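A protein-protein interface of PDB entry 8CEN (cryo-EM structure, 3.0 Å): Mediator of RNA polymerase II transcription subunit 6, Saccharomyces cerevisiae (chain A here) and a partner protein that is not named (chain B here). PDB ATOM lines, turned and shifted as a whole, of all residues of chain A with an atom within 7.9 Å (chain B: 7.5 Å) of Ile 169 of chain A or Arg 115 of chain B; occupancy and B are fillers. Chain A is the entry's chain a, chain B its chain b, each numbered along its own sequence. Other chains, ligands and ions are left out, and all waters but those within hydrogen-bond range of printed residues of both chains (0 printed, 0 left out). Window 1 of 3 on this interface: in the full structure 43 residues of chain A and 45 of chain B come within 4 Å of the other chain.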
ATOM      1  N   ASP A   7      29.870   8.934   1.910  1.00  0.00           N
ATOM      2  CA  ASP A   7      29.580  10.054   2.798  1.00  0.00           C
ATOM      3  C   ASP A   7      29.120   9.619   4.185  1.00  0.00           C
ATOM      4  O   ASP A   7      28.714  10.470   4.980  1.00  0.00           O
ATOM      5  CB  ASP A   7      28.513  10.943   2.152  1.00  0.00           C
ATOM      6  CG  ASP A   7      28.657  12.405   2.520  1.00  0.00           C
ATOM      7  OD1 ASP A   7      29.686  12.785   3.109  1.00  0.00           O
ATOM      8  OD2 ASP A   7      27.735  13.183   2.196  1.00  0.00           O
ATOM      9  N   GLU A   8      29.208   8.328   4.507  1.00  0.00           N
ATOM     10  CA  GLU A   8      28.513   7.788   5.667  1.00  0.00           C
ATOM     11  C   GLU A   8      29.414   6.855   6.476  1.00  0.00           C
ATOM     12  O   GLU A   8      28.921   6.142   7.356  1.00  0.00           O
ATOM     13  CB  GLU A   8      27.232   7.082   5.169  1.00  0.00           C
ATOM     14  CG  GLU A   8      26.128   6.767   6.178  1.00  0.00           C
ATOM     15  CD  GLU A   8      24.850   6.344   5.487  1.00  0.00           C
ATOM     16  OE1 GLU A   8      24.787   6.491   4.254  1.00  0.00           O
ATOM     17  OE2 GLU A   8      23.913   5.859   6.149  1.00  0.00           O
ATOM     18  N   TYR A 154      37.111  15.872   7.238  1.00  0.00           N
ATOM     19  CA  TYR A 154      37.715  16.275   8.499  1.00  0.00           C
ATOM     20  C   TYR A 154      38.331  15.080   9.213  1.00  0.00           C
ATOM     21  O   TYR A 154      37.793  13.967   9.185  1.00  0.00           O
ATOM     22  CB  TYR A 154      36.719  17.004   9.410  1.00  0.00           C
ATOM     23  CG  TYR A 154      35.428  16.293   9.738  1.00  0.00           C
ATOM     24  CD1 TYR A 154      34.350  16.331   8.864  1.00  0.00           C
ATOM     25  CD2 TYR A 154      35.267  15.635  10.948  1.00  0.00           C
ATOM     26  CE1 TYR A 154      33.161  15.703   9.171  1.00  0.00           C
ATOM     27  CE2 TYR A 154      34.081  15.005  11.266  1.00  0.00           C
ATOM     28  CZ  TYR A 154      33.031  15.044  10.374  1.00  0.00           C
ATOM     29  OH  TYR A 154      31.850  14.415  10.683  1.00  0.00           O
ATOM     30  N   GLN A 162      34.057  12.081   5.831  1.00  0.00           N
ATOM     31  CA  GLN A 162      33.657  12.944   4.729  1.00  0.00           C
ATOM     32  C   GLN A 162      32.539  13.861   5.196  1.00  0.00           C
ATOM     33  O   GLN A 162      31.555  13.397   5.779  1.00  0.00           O
ATOM     34  CB  GLN A 162      33.198  12.127   3.524  1.00  0.00           C
ATOM     35  CG  GLN A 162      32.837  12.978   2.326  1.00  0.00           C
ATOM     36  CD  GLN A 162      32.457  12.155   1.120  1.00  0.00           C
ATOM     37  OE1 GLN A 162      32.452  10.928   1.167  1.00  0.00           O
ATOM     38  NE2 GLN A 162      32.132  12.828   0.028  1.00  0.00           N
ATOM     39  N   SER A 163      32.701  15.162   4.951  1.00  0.00           N
ATOM     40  CA  SER A 163      31.751  16.199   5.314  1.00  0.00           C
ATOM     41  C   SER A 163      30.427  15.977   4.598  1.00  0.00           C
ATOM     42  O   SER A 163      30.346  16.141   3.375  1.00  0.00           O
ATOM     43  CB  SER A 163      32.317  17.575   4.963  1.00  0.00           C
ATOM     44  OG  SER A 163      33.276  17.989   5.917  1.00  0.00           O
ATOM     45  N   PRO A 164      29.378  15.600   5.317  1.00  0.00           N
ATOM     46  CA  PRO A 164      28.089  15.362   4.671  1.00  0.00           C
ATOM     47  C   PRO A 164      27.381  16.671   4.378  1.00  0.00           C
ATOM     48  O   PRO A 164      27.701  17.724   4.931  1.00  0.00           O
ATOM     49  CB  PRO A 164      27.326  14.541   5.712  1.00  0.00           C
ATOM     50  CG  PRO A 164      27.872  15.024   7.003  1.00  0.00           C
ATOM     51  CD  PRO A 164      29.294  15.453   6.780  1.00  0.00           C
ATOM     52  N   THR A 165      26.407  16.593   3.481  1.00  0.00           N
ATOM     53  CA  THR A 165      25.595  17.762   3.197  1.00  0.00           C
ATOM     54  C   THR A 165      24.585  17.960   4.319  1.00  0.00           C
ATOM     55  O   THR A 165      24.060  16.996   4.893  1.00  0.00           O
ATOM     56  CB  THR A 165      24.890  17.635   1.847  1.00  0.00           C
ATOM     57  OG1 THR A 165      23.860  16.649   1.925  1.00  0.00           O
ATOM     58  CG2 THR A 165      25.887  17.224   0.778  1.00  0.00           C
ATOM     59  N   ILE A 166      24.342  19.229   4.645  1.00  0.00           N
ATOM     60  CA  ILE A 166      23.452  19.564   5.746  1.00  0.00           C
ATOM     61  C   ILE A 166      22.017  19.150   5.430  1.00  0.00           C
ATOM     62  O   ILE A 166      21.251  18.806   6.345  1.00  0.00           O
ATOM     63  CB  ILE A 166      23.613  21.060   6.081  1.00  0.00           C
ATOM     64  CG1 ILE A 166      23.227  21.944   4.907  1.00  0.00           C
ATOM     65  CG2 ILE A 166      25.055  21.371   6.390  1.00  0.00           C
ATOM     66  CD1 ILE A 166      23.158  23.412   5.274  1.00  0.00           C
ATOM     67  N   PHE A 167      21.657  19.116   4.139  1.00  0.00           N
ATOM     68  CA  PHE A 167      20.420  18.469   3.705  1.00  0.00           C
ATOM     69  C   PHE A 167      20.379  17.017   4.149  1.00  0.00           C
ATOM     70  O   PHE A 167      19.368  16.558   4.683  1.00  0.00           O
ATOM     71  CB  PHE A 167      20.281  18.538   2.182  1.00  0.00           C
ATOM     72  CG  PHE A 167      18.971  17.988   1.649  1.00  0.00           C
ATOM     73  CD1 PHE A 167      18.842  16.646   1.305  1.00  0.00           C
ATOM     74  CD2 PHE A 167      17.876  18.814   1.480  1.00  0.00           C
ATOM     75  CE1 PHE A 167      17.649  16.144   0.822  1.00  0.00           C
ATOM     76  CE2 PHE A 167      16.681  18.314   0.985  1.00  0.00           C
ATOM     77  CZ  PHE A 167      16.568  16.978   0.666  1.00  0.00           C
ATOM     78  N   LYS A 168      21.461  16.272   3.902  1.00  0.00           N
ATOM     79  CA  LYS A 168      21.483  14.852   4.238  1.00  0.00           C
ATOM     80  C   LYS A 168      21.377  14.645   5.742  1.00  0.00           C
ATOM     81  O   LYS A 168      20.671  13.739   6.202  1.00  0.00           O
ATOM     82  CB  LYS A 168      22.757  14.206   3.695  1.00  0.00           C
ATOM     83  CG  LYS A 168      22.635  13.641   2.286  1.00  0.00           C
ATOM     84  CD  LYS A 168      21.537  12.606   2.183  1.00  0.00           C
ATOM     85  CE  LYS A 168      21.636  11.829   0.881  1.00  0.00           C
ATOM     86  NZ  LYS A 168      23.037  11.415   0.590  1.00  0.00           N
ATOM     87  N   ILE A 169      22.041  15.507   6.520  1.00  0.00           N
ATOM     88  CA  ILE A 169      21.992  15.401   7.980  1.00  0.00           C
ATOM     89  C   ILE A 169      20.571  15.623   8.492  1.00  0.00           C
ATOM     90  O   ILE A 169      19.994  14.766   9.184  1.00  0.00           O
ATOM     91  CB  ILE A 169      22.972  16.395   8.627  1.00  0.00           C
ATOM     92  CG1 ILE A 169      24.416  16.017   8.304  1.00  0.00           C
ATOM     93  CG2 ILE A 169      22.763  16.449  10.132  1.00  0.00           C
ATOM     94  CD1 ILE A 169      25.415  17.027   8.802  1.00  0.00           C
ATOM     95  N   VAL A 170      19.979  16.775   8.149  1.00  0.00           N
ATOM     96  CA  VAL A 170      18.651  17.078   8.669  1.00  0.00           C
ATOM     97  C   VAL A 170      17.604  16.161   8.059  1.00  0.00           C
ATOM     98  O   VAL A 170      16.589  15.872   8.698  1.00  0.00           O
ATOM     99  CB  VAL A 170      18.279  18.558   8.451  1.00  0.00           C
ATOM    100  CG1 VAL A 170      19.300  19.451   9.114  1.00  0.00           C
ATOM    101  CG2 VAL A 170      18.119  18.899   6.979  1.00  0.00           C
ATOM    102  N   GLN A 171      17.866  15.632   6.864  1.00  0.00           N
ATOM    103  CA  GLN A 171      16.925  14.742   6.208  1.00  0.00           C
ATOM    104  C   GLN A 171      16.912  13.377   6.876  1.00  0.00           C
ATOM    105  O   GLN A 171      15.845  12.798   7.070  1.00  0.00           O
ATOM    106  CB  GLN A 171      17.287  14.645   4.728  1.00  0.00           C
ATOM    107  CG  GLN A 171      16.430  13.726   3.899  1.00  0.00           C
ATOM    108  CD  GLN A 171      17.207  13.078   2.781  1.00  0.00           C
ATOM    109  OE1 GLN A 171      18.399  12.819   2.913  1.00  0.00           O
ATOM    110  NE2 GLN A 171      16.550  12.866   1.651  1.00  0.00           N
ATOM    111  N   SER A 172      18.086  12.857   7.252  1.00  0.00           N
ATOM    112  CA  SER A 172      18.135  11.610   8.012  1.00  0.00           C
ATOM    113  C   SER A 172      17.488  11.770   9.382  1.00  0.00           C
ATOM    114  O   SER A 172      16.756  10.878   9.843  1.00  0.00           O
ATOM    115  CB  SER A 172      19.582  11.149   8.161  1.00  0.00           C
ATOM    116  OG  SER A 172      20.336  12.090   8.903  1.00  0.00           O
ATOM    117  N   ARG A 173      17.743  12.906  10.042  1.00  0.00           N
ATOM    118  CA  ARG A 173      17.111  13.162  11.334  1.00  0.00           C
ATOM    119  C   ARG A 173      15.593  13.241  11.207  1.00  0.00           C
ATOM    120  O   ARG A 173      14.862  12.734  12.065  1.00  0.00           O
ATOM    121  CB  ARG A 173      17.661  14.447  11.940  1.00  0.00           C
ATOM    122  CG  ARG A 173      19.104  14.384  12.404  1.00  0.00           C
ATOM    123  CD  ARG A 173      19.321  13.273  13.414  1.00  0.00           C
ATOM    124  NE  ARG A 173      20.639  13.359  14.028  1.00  0.00           N
ATOM    125  CZ  ARG A 173      21.113  12.492  14.912  1.00  0.00           C
ATOM    126  NH1 ARG A 173      20.409  11.441  15.296  1.00  0.00           N
ATOM    127  NH2 ARG A 173      22.324  12.688  15.426  1.00  0.00           N
ATOM    128  N   LEU A 174      15.099  13.850  10.128  1.00  0.00           N
ATOM    129  CA  LEU A 174      13.658  13.941   9.931  1.00  0.00           C
ATOM    130  C   LEU A 174      13.045  12.624   9.459  1.00  0.00           C
ATOM    131  O   LEU A 174      11.869  12.379   9.732  1.00  0.00           O
ATOM    132  CB  LEU A 174      13.339  15.076   8.959  1.00  0.00           C
ATOM    133  CG  LEU A 174      13.469  16.474   9.571  1.00  0.00           C
ATOM    134  CD1 LEU A 174      13.385  17.557   8.509  1.00  0.00           C
ATOM    135  CD2 LEU A 174      12.408  16.687  10.640  1.00  0.00           C
ATOM    136  N   MET A 175      13.808  11.765   8.772  1.00  0.00           N
ATOM    137  CA  MET A 175      13.359  10.390   8.540  1.00  0.00           C
ATOM    138  C   MET A 175      13.152   9.651   9.852  1.00  0.00           C
ATOM    139  O   MET A 175      12.141   8.963  10.038  1.00  0.00           O
ATOM    140  CB  MET A 175      14.355   9.620   7.668  1.00  0.00           C
ATOM    141  CG  MET A 175      14.497  10.090   6.243  1.00  0.00           C
ATOM    142  SD  MET A 175      12.930   9.930   5.388  1.00  0.00           S
ATOM    143  CE  MET A 175      12.809   8.148   5.298  1.00  0.00           C
ATOM    144  N   SER A 176      14.113   9.776  10.771  1.00  0.00           N
ATOM    145  CA  SER A 176      13.965   9.138  12.077  1.00  0.00           C
ATOM    146  C   SER A 176      12.777   9.715  12.841  1.00  0.00           C
ATOM    147  O   SER A 176      11.998   8.970  13.453  1.00  0.00           O
ATOM    148  CB  SER A 176      15.253   9.292  12.880  1.00  0.00           C
ATOM    149  OG  SER A 176      16.346   8.680  12.220  1.00  0.00           O
ATOM    150  N   LEU B  83      12.516  22.585   3.410  1.00  0.00           N
ATOM    151  CA  LEU B  83      13.755  21.938   3.003  1.00  0.00           C
ATOM    152  C   LEU B  83      13.707  21.534   1.529  1.00  0.00           C
ATOM    153  O   LEU B  83      14.732  21.565   0.838  1.00  0.00           O
ATOM    154  CB  LEU B  83      13.996  20.736   3.913  1.00  0.00           C
ATOM    155  CG  LEU B  83      15.258  19.902   3.780  1.00  0.00           C
ATOM    156  CD1 LEU B  83      16.468  20.770   4.090  1.00  0.00           C
ATOM    157  CD2 LEU B  83      15.200  18.692   4.691  1.00  0.00           C
ATOM    158  N   LEU B  90      21.607  23.176  -0.160  1.00  0.00           N
ATOM    159  CA  LEU B  90      21.614  22.301   1.005  1.00  0.00           C
ATOM    160  C   LEU B  90      22.283  20.971   0.704  1.00  0.00           C
ATOM    161  O   LEU B  90      23.005  20.441   1.553  1.00  0.00           O
ATOM    162  CB  LEU B  90      20.171  22.074   1.495  1.00  0.00           C
ATOM    163  CG  LEU B  90      19.439  22.950   2.530  1.00  0.00           C
ATOM    164  CD1 LEU B  90      19.856  22.682   3.945  1.00  0.00           C
ATOM    165  CD2 LEU B  90      19.621  24.432   2.225  1.00  0.00           C
ATOM    166  N   ASP B  91      22.055  20.414  -0.492  1.00  0.00           N
ATOM    167  CA  ASP B  91      22.944  19.396  -1.045  1.00  0.00           C
ATOM    168  C   ASP B  91      24.255  19.987  -1.534  1.00  0.00           C
ATOM    169  O   ASP B  91      25.221  19.243  -1.730  1.00  0.00           O
ATOM    170  CB  ASP B  91      22.279  18.662  -2.213  1.00  0.00           C
ATOM    171  CG  ASP B  91      21.137  17.783  -1.776  1.00  0.00           C
ATOM    172  OD1 ASP B  91      21.185  17.294  -0.635  1.00  0.00           O
ATOM    173  OD2 ASP B  91      20.198  17.579  -2.572  1.00  0.00           O
ATOM    174  N   THR B  93      26.066  22.354   0.042  1.00  0.00           N
ATOM    175  CA  THR B  93      26.920  22.802   1.136  1.00  0.00           C
ATOM    176  C   THR B  93      27.229  21.614   2.031  1.00  0.00           C
ATOM    177  O   THR B  93      26.310  20.976   2.556  1.00  0.00           O
ATOM    178  CB  THR B  93      26.263  23.925   1.947  1.00  0.00           C
ATOM    179  OG1 THR B  93      25.045  23.448   2.530  1.00  0.00           O
ATOM    180  CG2 THR B  93      25.970  25.132   1.070  1.00  0.00           C
ATOM    181  N   VAL B  94      28.514  21.323   2.207  1.00  0.00           N
ATOM    182  CA  VAL B  94      28.978  20.279   3.112  1.00  0.00           C
ATOM    183  C   VAL B  94      29.598  20.954   4.327  1.00  0.00           C
ATOM    184  O   VAL B  94      30.187  22.035   4.218  1.00  0.00           O
ATOM    185  CB  VAL B  94      29.961  19.312   2.417  1.00  0.00           C
ATOM    186  CG1 VAL B  94      29.337  18.764   1.145  1.00  0.00           C
ATOM    187  CG2 VAL B  94      31.289  19.988   2.089  1.00  0.00           C
ATOM    188  N   VAL B  95      29.426  20.339   5.494  1.00  0.00           N
ATOM    189  CA  VAL B  95      29.757  20.973   6.763  1.00  0.00           C
ATOM    190  C   VAL B  95      30.891  20.215   7.445  1.00  0.00           C
ATOM    191  O   VAL B  95      30.914  18.979   7.469  1.00  0.00           O
ATOM    192  CB  VAL B  95      28.510  21.097   7.671  1.00  0.00           C
ATOM    193  CG1 VAL B  95      27.945  19.740   8.077  1.00  0.00           C
ATOM    194  CG2 VAL B  95      28.829  21.918   8.897  1.00  0.00           C
ATOM    195  N   LEU B 109      30.350  13.628  20.200  1.00  0.00           N
ATOM    196  CA  LEU B 109      29.358  14.690  20.070  1.00  0.00           C
ATOM    197  C   LEU B 109      29.346  15.266  18.657  1.00  0.00           C
ATOM    198  O   LEU B 109      28.273  15.463  18.073  1.00  0.00           O
ATOM    199  CB  LEU B 109      29.623  15.779  21.116  1.00  0.00           C
ATOM    200  CG  LEU B 109      28.632  16.927  21.353  1.00  0.00           C
ATOM    201  CD1 LEU B 109      28.731  17.377  22.795  1.00  0.00           C
ATOM    202  CD2 LEU B 109      28.884  18.125  20.445  1.00  0.00           C
ATOM    203  N   VAL B 110      30.525  15.534  18.085  1.00  0.00           N
ATOM    204  CA  VAL B 110      30.554  16.129  16.750  1.00  0.00           C
ATOM    205  C   VAL B 110      30.085  15.124  15.696  1.00  0.00           C
ATOM    206  O   VAL B 110      29.382  15.491  14.748  1.00  0.00           O
ATOM    207  CB  VAL B 110      31.942  16.726  16.427  1.00  0.00           C
ATOM    208  CG1 VAL B 110      33.040  15.682  16.398  1.00  0.00           C
ATOM    209  CG2 VAL B 110      31.908  17.507  15.118  1.00  0.00           C
ATOM    210  N   THR B 111      30.411  13.837  15.863  1.00  0.00           N
ATOM    211  CA  THR B 111      29.945  12.846  14.899  1.00  0.00           C
ATOM    212  C   THR B 111      28.450  12.581  15.030  1.00  0.00           C
ATOM    213  O   THR B 111      27.777  12.347  14.020  1.00  0.00           O
ATOM    214  CB  THR B 111      30.730  11.546  15.049  1.00  0.00           C
ATOM    215  OG1 THR B 111      30.684  11.106  16.411  1.00  0.00           O
ATOM    216  CG2 THR B 111      32.169  11.753  14.621  1.00  0.00           C
ATOM    217  N   THR B 112      27.912  12.614  16.253  1.00  0.00           N
ATOM    218  CA  THR B 112      26.472  12.489  16.437  1.00  0.00           C
ATOM    219  C   THR B 112      25.742  13.686  15.840  1.00  0.00           C
ATOM    220  O   THR B 112      24.685  13.534  15.215  1.00  0.00           O
ATOM    221  CB  THR B 112      26.159  12.331  17.931  1.00  0.00           C
ATOM    222  OG1 THR B 112      26.601  11.042  18.375  1.00  0.00           O
ATOM    223  CG2 THR B 112      24.668  12.460  18.210  1.00  0.00           C
ATOM    224  N   LEU B 113      26.309  14.883  15.985  1.00  0.00           N
ATOM    225  CA  LEU B 113      25.661  16.069  15.446  1.00  0.00           C
ATOM    226  C   LEU B 113      25.831  16.204  13.936  1.00  0.00           C
ATOM    227  O   LEU B 113      25.031  16.895  13.300  1.00  0.00           O
ATOM    228  CB  LEU B 113      26.196  17.316  16.150  1.00  0.00           C
ATOM    229  CG  LEU B 113      25.215  18.478  16.311  1.00  0.00           C
ATOM    230  CD1 LEU B 113      23.859  17.977  16.784  1.00  0.00           C
ATOM    231  CD2 LEU B 113      25.770  19.480  17.296  1.00  0.00           C
ATOM    232  N   LEU B 114      26.847  15.568  13.349  1.00  0.00           N
ATOM    233  CA  LEU B 114      27.069  15.626  11.910  1.00  0.00           C
ATOM    234  C   LEU B 114      26.782  14.311  11.199  1.00  0.00           C
ATOM    235  O   LEU B 114      27.178  14.153  10.041  1.00  0.00           O
ATOM    236  CB  LEU B 114      28.504  16.060  11.602  1.00  0.00           C
ATOM    237  CG  LEU B 114      28.953  17.426  12.111  1.00  0.00           C
ATOM    238  CD1 LEU B 114      30.385  17.706  11.692  1.00  0.00           C
ATOM    239  CD2 LEU B 114      28.026  18.492  11.584  1.00  0.00           C
ATOM    240  N   ARG B 115      26.128  13.358  11.854  1.00  0.00           N
ATOM    241  CA  ARG B 115      25.825  12.103  11.184  1.00  0.00           C
ATOM    242  C   ARG B 115      24.725  12.297  10.146  1.00  0.00           C
ATOM    243  O   ARG B 115      23.759  13.036  10.358  1.00  0.00           O
ATOM    244  CB  ARG B 115      25.438  11.028  12.206  1.00  0.00           C
ATOM    245  CG  ARG B 115      24.145  11.280  12.959  1.00  0.00           C
ATOM    246  CD  ARG B 115      23.657  10.057  13.719  1.00  0.00           C
ATOM    247  NE  ARG B 115      23.285   8.940  12.861  1.00  0.00           N
ATOM    248  CZ  ARG B 115      22.948   7.740  13.313  1.00  0.00           C
ATOM    249  NH1 ARG B 115      22.955   7.461  14.605  1.00  0.00           N
ATOM    250  NH2 ARG B 115      22.595   6.796  12.446  1.00  0.00           N
ATOM    251  N   LYS B 116      24.907  11.659   8.992  1.00  0.00           N
ATOM    252  CA  LYS B 116      23.886  11.597   7.959  1.00  0.00           C
ATOM    253  C   LYS B 116      23.286  10.208   7.835  1.00  0.00           C
ATOM    254  O   LYS B 116      22.390  10.001   7.013  1.00  0.00           O
ATOM    255  CB  LYS B 116      24.459  12.028   6.607  1.00  0.00           C
ATOM    256  CG  LYS B 116      25.421  11.025   6.007  1.00  0.00           C
ATOM    257  CD  LYS B 116      25.600  11.253   4.521  1.00  0.00           C
ATOM    258  CE  LYS B 116      24.385  10.778   3.755  1.00  0.00           C
ATOM    259  NZ  LYS B 116      24.097   9.345   4.019  1.00  0.00           N
ATOM    260  N   LYS B 117      23.777   9.249   8.612  1.00  0.00           N
ATOM    261  CA  LYS B 117      23.161   7.935   8.656  1.00  0.00           C
ATOM    262  C   LYS B 117      21.864   8.000   9.444  1.00  0.00           C
ATOM    263  O   LYS B 117      21.820   8.534  10.557  1.00  0.00           O
ATOM    264  CB  LYS B 117      24.124   6.923   9.276  1.00  0.00           C
ATOM    265  CG  LYS B 117      23.608   5.498   9.338  1.00  0.00           C
ATOM    266  CD  LYS B 117      24.629   4.562   9.956  1.00  0.00           C
ATOM    267  CE  LYS B 117      25.817   4.319   9.034  1.00  0.00           C
ATOM    268  NZ  LYS B 117      25.449   3.490   7.855  1.00  0.00           N
ATOM    269  N   ASN B 118      20.804   7.487   8.850  1.00  0.00           N
ATOM    270  CA  ASN B 118      19.552   7.244   9.544  1.00  0.00           C
ATOM    271  C   ASN B 118      19.459   5.794  10.005  1.00  0.00           C
ATOM    272  O   ASN B 118      20.236   4.931   9.587  1.00  0.00           O
ATOM    273  CB  ASN B 118      18.367   7.685   8.667  1.00  0.00           C
ATOM    274  CG  ASN B 118      18.263   6.921   7.361  1.00  0.00           C
ATOM    275  OD1 ASN B 118      18.989   5.970   7.109  1.00  0.00           O
ATOM    276  ND2 ASN B 118      17.347   7.361   6.512  1.00  0.00           N
ATOM    277  N   ILE B 119      18.490   5.544  10.878  1.00  0.00           N
ATOM    278  CA  ILE B 119      18.476   4.385  11.767  1.00  0.00           C
ATOM    279  C   ILE B 119      18.264   3.085  10.995  1.00  0.00           C
ATOM    280  O   ILE B 119      17.702   3.095   9.884  1.00  0.00           O
ATOM    281  CB  ILE B 119      17.418   4.574  12.868  1.00  0.00           C
ATOM    282  CG1 ILE B 119      16.010   4.570  12.273  1.00  0.00           C
ATOM    283  CG2 ILE B 119      17.688   5.859  13.638  1.00  0.00           C
ATOM    284  CD1 ILE B 119      14.917   4.794  13.276  1.00  0.00           C
ATOM    285  N   PRO B 120      18.747   1.953  11.522  1.00  0.00           N
ATOM    286  CA  PRO B 120      18.510   0.671  10.847  1.00  0.00           C
ATOM    287  C   PRO B 120      17.044   0.302  10.732  1.00  0.00           C
ATOM    288  O   PRO B 120      16.687  -0.428   9.804  1.00  0.00           O
ATOM    289  CB  PRO B 120      19.278  -0.331  11.721  1.00  0.00           C
ATOM    290  CG  PRO B 120      19.482   0.372  13.021  1.00  0.00           C
ATOM    291  CD  PRO B 120      19.683   1.792  12.645  1.00  0.00           C
ATOM    292  N   ASP B 123      15.965   2.174   7.605  1.00  0.00           N
ATOM    293  CA  ASP B 123      16.582   1.573   6.420  1.00  0.00           C
ATOM    294  C   ASP B 123      16.037   0.188   6.099  1.00  0.00           C
ATOM    295  O   ASP B 123      15.832  -0.131   4.920  1.00  0.00           O
ATOM    296  CB  ASP B 123      18.101   1.531   6.570  1.00  0.00           C
ATOM    297  CG  ASP B 123      18.712   2.900   6.504  1.00  0.00           C
ATOM    298  OD1 ASP B 123      18.104   3.740   5.806  1.00  0.00           O
ATOM    299  OD2 ASP B 123      19.751   3.148   7.152  1.00  0.00           O
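The side-chain carboxylate (OE1) of Glu 8 of chain A lies within salt-bridge range of the side-chain amino group (NZ) of Lys 116 of chain B (2.9 Å).
The backbone carbonyl oxygen (O) of Pro 164 of chain A sits at hydrogen-bond distance from the backbone NH (N) of Val 95 of chain B (3.2 Å).
O of Val 95 of chain B is in hydrogen-bond range of OG of Ser 163 of chain A (3.0 Å).
The side-chain carboxylate (OE2) of Glu 8 of chain A lies within salt-bridge range of the side-chain amino group (NZ) of Lys 117 of chain B, 3.3 Å away.
The side-chain hydroxyl (OG) of Ser 172 of chain A sits close to the backbone carbonyl oxygen (O) of Lys 116 of chain B, 3.5 Å away.
The backbone NH of Ile 166 of chain A lies within hydrogen-bond range of the backbone carbonyl oxygen of Thr 93 of chain B (3.4 Å).
NH2 of Arg 173 of chain A is in hydrogen-bond range of O of Thr 112 of chain B, 2.5 Å away.
N of Phe 167 of chain A lies within hydrogen-bond range of O of Leu 90 of chain B, 3.2 Å away.
The guanidinium group (NH2) of Arg 115 of chain B lies within hydrogen-bond range of the backbone carbonyl oxygen (O) of Lys 117 of chain B (2.7 Å).
OE1 of Gln 162 of chain A sits at hydrogen-bond distance from N of Asp 7 of chain A.
Among the printed residues, pairs that only touch across the chains: Asp 7 of chain A with Lys 116 of chain B (3.2 Å), Tyr 154 of chain A with Leu 114 of chain B (3.7 Å), Ser 163 of chain A with Val 94 of chain B (3.3 Å), Pro 164 of chain A with Val 94 of chain B (3.4 Å), Pro 164 of chain A with Leu 114 of chain B (3.2 Å), Pro 164 of chain A with Lys 116 of chain B (3.9 Å), Thr 165 of chain A with Leu 90 of chain B (3.4 Å), Thr 165 of chain A with Asp 91 of chain B (3.3 Å), Thr 165 of chain A with Thr 93 of chain B (3.4 Å), Thr 165 of chain A with Val 94 of chain B (3.8 Å), Ile 166 of chain A with Leu 90 of chain B (3.6 Å), Ile 166 of chain A with Val 95 of chain B (3.7 Å), Phe 167 of chain A with Leu 83 of chain B (3.5 Å), Phe 167 of chain A with Asp 91 of chain B (3.1 Å), Lys 168 of chain A with Lys 116 of chain B (3.5 Å), Ile 169 of chain A with Val 95 of chain B (3.8 Å), Ile 169 of chain A with Leu 113 of chain B (3.9 Å), Ile 169 of chain A with Leu 114 of chain B (3.6 Å), Ile 169 of chain A with Arg 115 of chain B (3.6 Å), Val 170 of chain A with Leu 83 of chain B (3.7 Å), Ser 172 of chain A with Arg 115 of chain B (3.8 Å), Ser 172 of chain A with Asn 118 of chain B (3.7 Å), Arg 173 of chain A with Arg 115 of chain B (3.4 Å), Met 175 of chain A with Asn 118 of chain B (3.9 Å) and Ser 176 of chain A with Ile 119 of chain B (3.4 Å).
Ile 169 of chain A touches just these residues of chain B: Val 95 (3.8 Å), Leu 113 (3.9 Å), Leu 114 (3.6 Å) and Arg 115 (3.6 Å).
Of the printed residues of chain A, Leu 114 of chain B touches Tyr 154, Pro 164 and Ile 169.
Of the printed residues of chain B, Arg 173 of chain A touches Thr 112 (2.5 Å) and Arg 115 (3.4 Å).
Of the printed residues of chain A, Asn 118 of chain B touches Ser 172 and Met 175.
Pro 120 of chain B touches none of the printed residues of chain A.
The nearest printed residue of chain A that does not touch Arg 115 of chain B is Pro 164 of chain A (5.2 Å).
Hydrophobic or aromatic side chains of chain B within 4 Å of the printed part of chain A: Leu 83, Leu 90, Val 94, Val 95, Leu 114 and Ile 119.
Among the printed residues, 33 pairs touch across the chains.
Among the printed residues, Asp or Glu carboxylates within 4 Å of a Lys or Arg side-chain nitrogen of the other chain: Glu 8 of chain A with Lys 116 of chain B and Glu 8 of chain A with Lys 117 of chain B.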
